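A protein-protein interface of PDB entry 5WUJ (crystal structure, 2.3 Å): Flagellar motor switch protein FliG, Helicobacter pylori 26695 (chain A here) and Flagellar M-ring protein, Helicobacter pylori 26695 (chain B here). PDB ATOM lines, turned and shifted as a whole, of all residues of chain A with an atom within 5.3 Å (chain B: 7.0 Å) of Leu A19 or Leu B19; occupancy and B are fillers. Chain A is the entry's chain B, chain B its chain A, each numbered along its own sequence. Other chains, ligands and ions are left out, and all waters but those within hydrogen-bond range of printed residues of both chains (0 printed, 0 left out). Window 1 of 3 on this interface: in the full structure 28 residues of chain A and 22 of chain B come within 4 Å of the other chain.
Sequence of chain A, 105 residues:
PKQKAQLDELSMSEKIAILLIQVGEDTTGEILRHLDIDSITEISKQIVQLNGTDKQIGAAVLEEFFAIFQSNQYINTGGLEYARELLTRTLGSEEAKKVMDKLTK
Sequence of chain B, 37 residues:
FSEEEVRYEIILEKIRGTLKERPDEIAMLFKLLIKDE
The guanidinium group (NH2) of Arg B16 is in hydrogen-bond range of the backbone carbonyl oxygen (O) of Gln A22 (3.5 Å). The side-chain hydroxyl (OG1) of Thr A27 lies within hydrogen-bond range of the side-chain amino group (NZ) of Lys B20 (2.9 Å). NE of Arg B16 sits at hydrogen-bond distance from O of Val A23, 2.9 Å away.
O of Ile A18 sits close to OE1 of Gln A22.
Among the printed residues, merely in contact across the chains: Leu A62 with Ile B15 (3.4 Å), Gln A22 with Leu B12 (3.5 Å), Ile A31 with Pro B23 (3.6 Å), Thr A27 with Arg B16 (3.6 Å), Thr A27 with Leu B19 (3.6 Å), Phe A65 with Phe B30 (3.7 Å), Ile A31 with Leu B19 (3.7 Å), Ile A16 with Phe B30 (3.7 Å), Leu A19 with Leu B19 (3.8 Å), Leu A20 with Leu B19 (3.9 Å), Ile A31 with Ala B27 (3.9 Å) and Leu A62 with Leu B12 (3.99 Å).
Of chain B, only Leu B19 comes within 4 Å of Leu A19. Of the printed residues of chain B, Gln A22 touches Leu B12 and Arg B16. Printed residues of chain B within 4 Å of Leu A62: Leu B12 (3.99 Å) and Ile B15 (3.4 Å). Of the printed residues of chain A, Leu B12 touches Gln A22 (3.5 Å) and Leu A62 (3.99 Å). Printed residues of chain A within 4 Å of Ile B15: Leu A62. The nearest residue of chain B that does not touch Leu A19 is Phe B30 (4.2 Å). The nearest printed residue of chain A that does not touch Arg B16 is Phe A69 (6.6 Å).
Printed residues of chain B that touch a printed residue of chain A: Leu B12, Ile B15, Arg B16, Leu B19, Lys B20, Pro B23, Ala B27 and Phe B30. Hydrophobic or aromatic side chains of chain B that line the printed part of chain A: Leu B12, Ile B15, Leu B19, Ala B27 and Phe B30. Printed residues of chain A that touch a printed residue of chain B: Ile A16, Leu A19, Leu A20, Gln A22, Val A23, Thr A27, Ile A31, Leu A62 and Phe A65. Hydrophobic or aromatic side chains of chain A that line the printed part of chain B: Ile A16, Leu A19, Leu A20, Ile A31, Leu A62 and Phe A65. Among the printed residues, no Asp or Glu carboxylate lies within 4 Å of a Lys or Arg side-chain nitrogen of the other chain.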
ATOM      1  N   GLU A  14      18.641 -33.376  16.063  1.00  0.00           N
ATOM      2  CA  GLU A  14      17.237 -33.092  16.373  1.00  0.00           C
ATOM      3  C   GLU A  14      16.810 -31.729  15.855  1.00  0.00           C
ATOM      4  O   GLU A  14      15.702 -31.580  15.321  1.00  0.00           O
ATOM      5  CB  GLU A  14      17.009 -33.174  17.879  1.00  0.00           C
ATOM      6  CG  GLU A  14      17.491 -34.506  18.441  1.00  0.00           C
ATOM      7  CD  GLU A  14      17.111 -34.697  19.873  1.00  0.00           C
ATOM      8  OE1 GLU A  14      17.777 -34.105  20.754  1.00  0.00           O
ATOM      9  OE2 GLU A  14      16.150 -35.449  20.112  1.00  0.00           O
ATOM     10  N   LYS A  15      17.667 -30.720  16.020  1.00  0.00           N
ATOM     11  CA  LYS A  15      17.372 -29.397  15.477  1.00  0.00           C
ATOM     12  C   LYS A  15      17.223 -29.453  13.966  1.00  0.00           C
ATOM     13  O   LYS A  15      16.350 -28.788  13.394  1.00  0.00           O
ATOM     14  CB  LYS A  15      18.474 -28.415  15.852  1.00  0.00           C
ATOM     15  CG  LYS A  15      18.671 -28.233  17.364  1.00  0.00           C
ATOM     16  CD  LYS A  15      19.403 -26.941  17.628  1.00  0.00           C
ATOM     17  CE  LYS A  15      19.743 -26.743  19.075  1.00  0.00           C
ATOM     18  NZ  LYS A  15      21.179 -26.375  19.174  1.00  0.00           N
ATOM     19  N   ILE A  16      18.053 -30.257  13.299  1.00  0.00           N
ATOM     20  CA  ILE A  16      17.986 -30.325  11.841  1.00  0.00           C
ATOM     21  C   ILE A  16      16.685 -30.979  11.396  1.00  0.00           C
ATOM     22  O   ILE A  16      16.039 -30.512  10.456  1.00  0.00           O
ATOM     23  CB  ILE A  16      19.221 -31.058  11.290  1.00  0.00           C
ATOM     24  CG1 ILE A  16      20.453 -30.153  11.359  1.00  0.00           C
ATOM     25  CG2 ILE A  16      18.971 -31.554   9.874  1.00  0.00           C
ATOM     26  CD1 ILE A  16      21.790 -30.935  11.301  1.00  0.00           C
ATOM     27  N   ALA A  17      16.259 -32.051  12.075  1.00  0.00           N
ATOM     28  CA  ALA A  17      14.976 -32.663  11.735  1.00  0.00           C
ATOM     29  C   ALA A  17      13.823 -31.706  12.005  1.00  0.00           C
ATOM     30  O   ALA A  17      12.868 -31.631  11.215  1.00  0.00           O
ATOM     31  CB  ALA A  17      14.781 -33.958  12.521  1.00  0.00           C
ATOM     32  N   ILE A  18      13.899 -30.947  13.105  1.00  0.00           N
ATOM     33  CA  ILE A  18      12.859 -29.955  13.371  1.00  0.00           C
ATOM     34  C   ILE A  18      12.848 -28.892  12.275  1.00  0.00           C
ATOM     35  O   ILE A  18      11.781 -28.476  11.804  1.00  0.00           O
ATOM     36  CB  ILE A  18      13.037 -29.346  14.778  1.00  0.00           C
ATOM     37  CG1 ILE A  18      12.460 -30.301  15.832  1.00  0.00           C
ATOM     38  CG2 ILE A  18      12.337 -28.005  14.888  1.00  0.00           C
ATOM     39  CD1 ILE A  18      13.127 -30.185  17.191  1.00  0.00           C
ATOM     40  N   LEU A  19      14.025 -28.445  11.832  1.00  0.00           N
ATOM     41  CA  LEU A  19      14.051 -27.546  10.677  1.00  0.00           C
ATOM     42  C   LEU A  19      13.400 -28.208   9.465  1.00  0.00           C
ATOM     43  O   LEU A  19      12.557 -27.600   8.792  1.00  0.00           O
ATOM     44  CB  LEU A  19      15.492 -27.119  10.365  1.00  0.00           C
ATOM     45  CG  LEU A  19      15.761 -26.162   9.195  1.00  0.00           C
ATOM     46  CD1 LEU A  19      17.091 -25.514   9.421  1.00  0.00           C
ATOM     47  CD2 LEU A  19      15.784 -26.870   7.844  1.00  0.00           C
ATOM     48  N   LEU A  20      13.764 -29.473   9.180  1.00  0.00           N
ATOM     49  CA  LEU A  20      13.241 -30.129   7.981  1.00  0.00           C
ATOM     50  C   LEU A  20      11.727 -30.296   8.043  1.00  0.00           C
ATOM     51  O   LEU A  20      11.024 -30.043   7.055  1.00  0.00           O
ATOM     52  CB  LEU A  20      13.923 -31.477   7.774  1.00  0.00           C
ATOM     53  CG  LEU A  20      15.376 -31.279   7.345  1.00  0.00           C
ATOM     54  CD1 LEU A  20      16.141 -32.599   7.353  1.00  0.00           C
ATOM     55  CD2 LEU A  20      15.436 -30.617   5.958  1.00  0.00           C
ATOM     56  N   ILE A  21      11.206 -30.712   9.193  1.00  0.00           N
ATOM     57  CA  ILE A  21       9.760 -30.811   9.367  1.00  0.00           C
ATOM     58  C   ILE A  21       9.085 -29.505   8.957  1.00  0.00           C
ATOM     59  O   ILE A  21       8.074 -29.501   8.248  1.00  0.00           O
ATOM     60  CB  ILE A  21       9.422 -31.179  10.827  1.00  0.00           C
ATOM     61  CG1 ILE A  21       9.846 -32.613  11.176  1.00  0.00           C
ATOM     62  CG2 ILE A  21       7.949 -30.915  11.123  1.00  0.00           C
ATOM     63  CD1 ILE A  21       9.869 -32.908  12.698  1.00  0.00           C
ATOM     64  N   GLN A  22       9.635 -28.373   9.387  1.00  0.00           N
ATOM     65  CA  GLN A  22       8.973 -27.106   9.106  1.00  0.00           C
ATOM     66  C   GLN A  22       9.100 -26.683   7.640  1.00  0.00           C
ATOM     67  O   GLN A  22       8.244 -25.943   7.150  1.00  0.00           O
ATOM     68  CB  GLN A  22       9.523 -26.018  10.013  1.00  0.00           C
ATOM     69  CG  GLN A  22       9.189 -26.205  11.478  1.00  0.00           C
ATOM     70  CD  GLN A  22      10.017 -25.280  12.335  1.00  0.00           C
ATOM     71  OE1 GLN A  22      11.176 -25.569  12.664  1.00  0.00           O
ATOM     72  NE2 GLN A  22       9.456 -24.135  12.648  1.00  0.00           N
ATOM     73  N   VAL A  23      10.149 -27.115   6.920  1.00  0.00           N
ATOM     74  CA  VAL A  23      10.228 -26.715   5.511  1.00  0.00           C
ATOM     75  C   VAL A  23       9.356 -27.580   4.611  1.00  0.00           C
ATOM     76  O   VAL A  23       9.077 -27.190   3.471  1.00  0.00           O
ATOM     77  CB  VAL A  23      11.672 -26.685   4.963  1.00  0.00           C
ATOM     78  CG1 VAL A  23      12.521 -25.656   5.725  1.00  0.00           C
ATOM     79  CG2 VAL A  23      12.325 -28.061   4.981  1.00  0.00           C
ATOM     80  N   THR A  27      10.913 -30.077   0.077  1.00  0.00           N
ATOM     81  CA  THR A  27      12.255 -29.554   0.298  1.00  0.00           C
ATOM     82  C   THR A  27      13.094 -30.525   1.110  1.00  0.00           C
ATOM     83  O   THR A  27      14.292 -30.679   0.854  1.00  0.00           O
ATOM     84  CB  THR A  27      12.159 -28.203   0.999  1.00  0.00           C
ATOM     85  OG1 THR A  27      11.365 -27.322   0.200  1.00  0.00           O
ATOM     86  CG2 THR A  27      13.532 -27.603   1.229  1.00  0.00           C
ATOM     87  N   ILE A  31      16.950 -32.416   0.360  1.00  0.00           N
ATOM     88  CA  ILE A  31      18.140 -32.537   1.202  1.00  0.00           C
ATOM     89  C   ILE A  31      18.524 -34.002   1.362  1.00  0.00           C
ATOM     90  O   ILE A  31      19.694 -34.378   1.186  1.00  0.00           O
ATOM     91  CB  ILE A  31      17.912 -31.890   2.578  1.00  0.00           C
ATOM     92  CG1 ILE A  31      17.762 -30.365   2.485  1.00  0.00           C
ATOM     93  CG2 ILE A  31      19.092 -32.204   3.483  1.00  0.00           C
ATOM     94  CD1 ILE A  31      18.761 -29.696   1.592  1.00  0.00           C
ATOM     95  N   VAL A  61      14.350 -22.811  16.705  1.00  0.00           N
ATOM     96  CA  VAL A  61      15.308 -23.535  15.866  1.00  0.00           C
ATOM     97  C   VAL A  61      15.540 -22.794  14.554  1.00  0.00           C
ATOM     98  O   VAL A  61      16.685 -22.629  14.111  1.00  0.00           O
ATOM     99  CB  VAL A  61      14.838 -24.986  15.623  1.00  0.00           C
ATOM    100  CG1 VAL A  61      15.686 -25.688  14.510  1.00  0.00           C
ATOM    101  CG2 VAL A  61      14.948 -25.793  16.902  1.00  0.00           C
ATOM    102  N   LEU A  62      14.462 -22.333  13.909  1.00  0.00           N
ATOM    103  CA  LEU A  62      14.620 -21.580  12.668  1.00  0.00           C
ATOM    104  C   LEU A  62      15.451 -20.324  12.886  1.00  0.00           C
ATOM    105  O   LEU A  62      16.296 -19.972  12.055  1.00  0.00           O
ATOM    106  CB  LEU A  62      13.255 -21.195  12.102  1.00  0.00           C
ATOM    107  CG  LEU A  62      12.417 -22.326  11.564  1.00  0.00           C
ATOM    108  CD1 LEU A  62      11.213 -21.756  10.811  1.00  0.00           C
ATOM    109  CD2 LEU A  62      13.270 -23.251  10.694  1.00  0.00           C
ATOM    110  N   PHE A  65      19.048 -21.261  12.915  1.00  0.00           N
ATOM    111  CA  PHE A  65      19.584 -21.525  11.583  1.00  0.00           C
ATOM    112  C   PHE A  65      19.600 -20.272  10.717  1.00  0.00           C
ATOM    113  O   PHE A  65      20.507 -20.115   9.895  1.00  0.00           O
ATOM    114  CB  PHE A  65      18.790 -22.627  10.911  1.00  0.00           C
ATOM    115  CG  PHE A  65      19.269 -23.988  11.290  1.00  0.00           C
ATOM    116  CD1 PHE A  65      20.360 -24.546  10.653  1.00  0.00           C
ATOM    117  CD2 PHE A  65      18.649 -24.696  12.305  1.00  0.00           C
ATOM    118  CE1 PHE A  65      20.826 -25.806  11.016  1.00  0.00           C
ATOM    119  CE2 PHE A  65      19.106 -25.963  12.665  1.00  0.00           C
ATOM    120  CZ  PHE A  65      20.195 -26.507  12.029  1.00  0.00           C
ATOM    121  N   PHE A  69      22.861 -19.059   8.592  1.00  0.00           N
ATOM    122  CA  PHE A  69      22.866 -18.749   7.171  1.00  0.00           C
ATOM    123  C   PHE A  69      23.224 -17.286   6.912  1.00  0.00           C
ATOM    124  O   PHE A  69      23.866 -16.978   5.900  1.00  0.00           O
ATOM    125  CB  PHE A  69      21.510 -19.098   6.569  1.00  0.00           C
ATOM    126  CG  PHE A  69      21.192 -20.564   6.600  1.00  0.00           C
ATOM    127  CD1 PHE A  69      22.200 -21.506   6.583  1.00  0.00           C
ATOM    128  CD2 PHE A  69      19.886 -21.005   6.622  1.00  0.00           C
ATOM    129  CE1 PHE A  69      21.906 -22.862   6.604  1.00  0.00           C
ATOM    130  CE2 PHE A  69      19.586 -22.364   6.640  1.00  0.00           C
ATOM    131  CZ  PHE A  69      20.603 -23.294   6.626  1.00  0.00           C
ATOM    132  N   LEU B  12      11.187 -18.551   7.715  1.00  0.00           N
ATOM    133  CA  LEU B  12      10.892 -19.842   7.091  1.00  0.00           C
ATOM    134  C   LEU B  12      11.041 -19.777   5.573  1.00  0.00           C
ATOM    135  O   LEU B  12      11.612 -20.684   4.954  1.00  0.00           O
ATOM    136  CB  LEU B  12       9.481 -20.313   7.455  1.00  0.00           C
ATOM    137  CG  LEU B  12       8.996 -21.623   6.807  1.00  0.00           C
ATOM    138  CD1 LEU B  12       9.889 -22.806   7.195  1.00  0.00           C
ATOM    139  CD2 LEU B  12       7.542 -21.931   7.177  1.00  0.00           C
ATOM    140  N   LYS B  14      12.855 -17.760   3.750  1.00  0.00           N
ATOM    141  CA  LYS B  14      14.244 -17.614   3.338  1.00  0.00           C
ATOM    142  C   LYS B  14      15.050 -18.868   3.611  1.00  0.00           C
ATOM    143  O   LYS B  14      15.952 -19.199   2.829  1.00  0.00           O
ATOM    144  CB  LYS B  14      14.870 -16.401   4.025  1.00  0.00           C
ATOM    145  CG  LYS B  14      14.251 -15.100   3.510  1.00  0.00           C
ATOM    146  CD  LYS B  14      15.012 -13.866   3.940  1.00  0.00           C
ATOM    147  CE  LYS B  14      14.205 -12.599   3.583  1.00  0.00           C
ATOM    148  NZ  LYS B  14      14.012 -12.480   2.111  1.00  0.00           N
ATOM    149  N   ILE B  15      14.731 -19.588   4.689  1.00  0.00           N
ATOM    150  CA  ILE B  15      15.420 -20.844   4.947  1.00  0.00           C
ATOM    151  C   ILE B  15      15.021 -21.883   3.902  1.00  0.00           C
ATOM    152  O   ILE B  15      15.875 -22.578   3.344  1.00  0.00           O
ATOM    153  CB  ILE B  15      15.140 -21.316   6.387  1.00  0.00           C
ATOM    154  CG1 ILE B  15      15.917 -20.440   7.391  1.00  0.00           C
ATOM    155  CG2 ILE B  15      15.481 -22.779   6.556  1.00  0.00           C
ATOM    156  CD1 ILE B  15      15.454 -20.581   8.851  1.00  0.00           C
ATOM    157  N   ARG B  16      13.723 -21.985   3.602  1.00  0.00           N
ATOM    158  CA  ARG B  16      13.279 -22.886   2.546  1.00  0.00           C
ATOM    159  C   ARG B  16      13.964 -22.550   1.233  1.00  0.00           C
ATOM    160  O   ARG B  16      14.472 -23.441   0.538  1.00  0.00           O
ATOM    161  CB  ARG B  16      11.760 -22.826   2.387  1.00  0.00           C
ATOM    162  CG  ARG B  16      11.166 -24.040   1.691  1.00  0.00           C
ATOM    163  CD  ARG B  16       9.672 -23.867   1.447  1.00  0.00           C
ATOM    164  NE  ARG B  16       8.891 -24.397   2.557  1.00  0.00           N
ATOM    165  CZ  ARG B  16       8.020 -23.690   3.268  1.00  0.00           C
ATOM    166  NH1 ARG B  16       7.810 -22.407   2.985  1.00  0.00           N
ATOM    167  NH2 ARG B  16       7.352 -24.268   4.257  1.00  0.00           N
ATOM    168  N   GLY B  17      14.012 -21.262   0.889  1.00  0.00           N
ATOM    169  CA  GLY B  17      14.672 -20.859  -0.348  1.00  0.00           C
ATOM    170  C   GLY B  17      16.137 -21.269  -0.399  1.00  0.00           C
ATOM    171  O   GLY B  17      16.638 -21.699  -1.440  1.00  0.00           O
ATOM    172  N   THR B  18      16.841 -21.148   0.726  1.00  0.00           N
ATOM    173  CA  THR B  18      18.253 -21.506   0.736  1.00  0.00           C
ATOM    174  C   THR B  18      18.435 -23.010   0.565  1.00  0.00           C
ATOM    175  O   THR B  18      19.325 -23.451  -0.170  1.00  0.00           O
ATOM    176  CB  THR B  18      18.914 -21.023   2.027  1.00  0.00           C
ATOM    177  OG1 THR B  18      19.162 -19.631   1.902  1.00  0.00           O
ATOM    178  CG2 THR B  18      20.250 -21.718   2.242  1.00  0.00           C
ATOM    179  N   LEU B  19      17.593 -23.809   1.224  1.00  0.00           N
ATOM    180  CA  LEU B  19      17.670 -25.258   1.055  1.00  0.00           C
ATOM    181  C   LEU B  19      17.411 -25.666  -0.391  1.00  0.00           C
ATOM    182  O   LEU B  19      18.115 -26.532  -0.931  1.00  0.00           O
ATOM    183  CB  LEU B  19      16.686 -25.952   1.994  1.00  0.00           C
ATOM    184  CG  LEU B  19      17.333 -26.404   3.304  1.00  0.00           C
ATOM    185  CD1 LEU B  19      17.759 -25.198   4.152  1.00  0.00           C
ATOM    186  CD2 LEU B  19      16.409 -27.327   4.078  1.00  0.00           C
ATOM    187  N   LYS B  20      16.430 -25.048  -1.036  1.00  0.00           N
ATOM    188  CA  LYS B  20      16.108 -25.381  -2.420  1.00  0.00           C
ATOM    189  C   LYS B  20      17.199 -24.973  -3.400  1.00  0.00           C
ATOM    190  O   LYS B  20      17.481 -25.683  -4.345  1.00  0.00           O
ATOM    191  CB  LYS B  20      14.774 -24.760  -2.837  1.00  0.00           C
ATOM    192  CG  LYS B  20      13.570 -25.472  -2.265  1.00  0.00           C
ATOM    193  CD  LYS B  20      12.280 -24.902  -2.813  1.00  0.00           C
ATOM    194  CE  LYS B  20      11.147 -25.904  -2.716  1.00  0.00           C
ATOM    195  NZ  LYS B  20      11.634 -27.310  -2.664  1.00  0.00           N
ATOM    196  N   GLU B  21      17.803 -23.824  -3.133  1.00  0.00           N
ATOM    197  CA  GLU B  21      18.862 -23.237  -3.934  1.00  0.00           C
ATOM    198  C   GLU B  21      20.113 -24.104  -4.059  1.00  0.00           C
ATOM    199  O   GLU B  21      20.630 -24.278  -5.148  1.00  0.00           O
ATOM    200  CB  GLU B  21      19.237 -21.888  -3.337  1.00  0.00           C
ATOM    201  CG  GLU B  21      19.831 -20.887  -4.303  1.00  0.00           C
ATOM    202  CD  GLU B  21      20.127 -19.556  -3.639  1.00  0.00           C
ATOM    203  OE1 GLU B  21      19.179 -18.898  -3.184  1.00  0.00           O
ATOM    204  OE2 GLU B  21      21.300 -19.170  -3.560  1.00  0.00           O
ATOM    205  N   ARG B  22      20.596 -24.639  -2.944  1.00  0.00           N
ATOM    206  CA  ARG B  22      21.778 -25.492  -2.948  1.00  0.00           C
ATOM    207  C   ARG B  22      21.604 -26.657  -1.995  1.00  0.00           C
ATOM    208  O   ARG B  22      22.164 -26.661  -0.918  1.00  0.00           O
ATOM    209  CB  ARG B  22      23.011 -24.692  -2.555  1.00  0.00           C
ATOM    210  CG  ARG B  22      22.750 -23.665  -1.480  1.00  0.00           C
ATOM    211  CD  ARG B  22      22.866 -22.276  -2.049  1.00  0.00           C
ATOM    212  NE  ARG B  22      24.255 -21.877  -2.124  1.00  0.00           N
ATOM    213  CZ  ARG B  22      24.684 -20.652  -1.889  1.00  0.00           C
ATOM    214  NH1 ARG B  22      23.826 -19.702  -1.578  1.00  0.00           N
ATOM    215  NH2 ARG B  22      25.972 -20.389  -1.963  1.00  0.00           N
ATOM    216  N   PRO B  23      20.844 -27.658  -2.413  1.00  0.00           N
ATOM    217  CA  PRO B  23      20.569 -28.798  -1.525  1.00  0.00           C
ATOM    218  C   PRO B  23      21.805 -29.598  -1.166  1.00  0.00           C
ATOM    219  O   PRO B  23      21.913 -30.071  -0.025  1.00  0.00           O
ATOM    220  CB  PRO B  23      19.567 -29.636  -2.338  1.00  0.00           C
ATOM    221  CG  PRO B  23      19.797 -29.230  -3.775  1.00  0.00           C
ATOM    222  CD  PRO B  23      20.060 -27.746  -3.656  1.00  0.00           C
ATOM    223  N   ASP B  24      22.745 -29.771  -2.102  1.00  0.00           N
ATOM    224  CA  ASP B  24      23.917 -30.575  -1.784  1.00  0.00           C
ATOM    225  C   ASP B  24      24.799 -29.866  -0.763  1.00  0.00           C
ATOM    226  O   ASP B  24      25.315 -30.501   0.161  1.00  0.00           O
ATOM    227  CB  ASP B  24      24.700 -30.936  -3.058  1.00  0.00           C
ATOM    228  CG  ASP B  24      25.112 -29.710  -3.884  1.00  0.00           C
ATOM    229  OD1 ASP B  24      24.450 -28.640  -3.769  1.00  0.00           O
ATOM    230  OD2 ASP B  24      26.097 -29.828  -4.662  1.00  0.00           O
ATOM    231  N   ILE B  26      23.809 -27.530   1.565  1.00  0.00           N
ATOM    232  CA  ILE B  26      23.153 -27.541   2.872  1.00  0.00           C
ATOM    233  C   ILE B  26      23.213 -28.931   3.493  1.00  0.00           C
ATOM    234  O   ILE B  26      23.431 -29.077   4.702  1.00  0.00           O
ATOM    235  CB  ILE B  26      21.697 -27.043   2.766  1.00  0.00           C
ATOM    236  CG1 ILE B  26      21.660 -25.623   2.212  1.00  0.00           C
ATOM    237  CG2 ILE B  26      21.055 -27.038   4.149  1.00  0.00           C
ATOM    238  CD1 ILE B  26      22.533 -24.646   2.979  1.00  0.00           C
ATOM    239  N   ALA B  27      23.024 -29.976   2.680  1.00  0.00           N
ATOM    240  CA  ALA B  27      23.153 -31.339   3.187  1.00  0.00           C
ATOM    241  C   ALA B  27      24.516 -31.562   3.825  1.00  0.00           C
ATOM    242  O   ALA B  27      24.624 -32.195   4.883  1.00  0.00           O
ATOM    243  CB  ALA B  27      22.932 -32.346   2.066  1.00  0.00           C
ATOM    244  N   PHE B  30      24.794 -29.699   7.054  1.00  0.00           N
ATOM    245  CA  PHE B  30      24.143 -30.425   8.139  1.00  0.00           C
ATOM    246  C   PHE B  30      25.048 -31.527   8.670  1.00  0.00           C
ATOM    247  O   PHE B  30      25.190 -31.694   9.888  1.00  0.00           O
ATOM    248  CB  PHE B  30      22.806 -31.006   7.670  1.00  0.00           C
ATOM    249  CG  PHE B  30      21.728 -29.988   7.487  1.00  0.00           C
ATOM    250  CD1 PHE B  30      21.783 -28.769   8.138  1.00  0.00           C
ATOM    251  CD2 PHE B  30      20.649 -30.250   6.648  1.00  0.00           C
ATOM    252  CE1 PHE B  30      20.760 -27.820   7.972  1.00  0.00           C
ATOM    253  CE2 PHE B  30      19.631 -29.326   6.480  1.00  0.00           C
ATOM    254  CZ  PHE B  30      19.687 -28.100   7.145  1.00  0.00           C
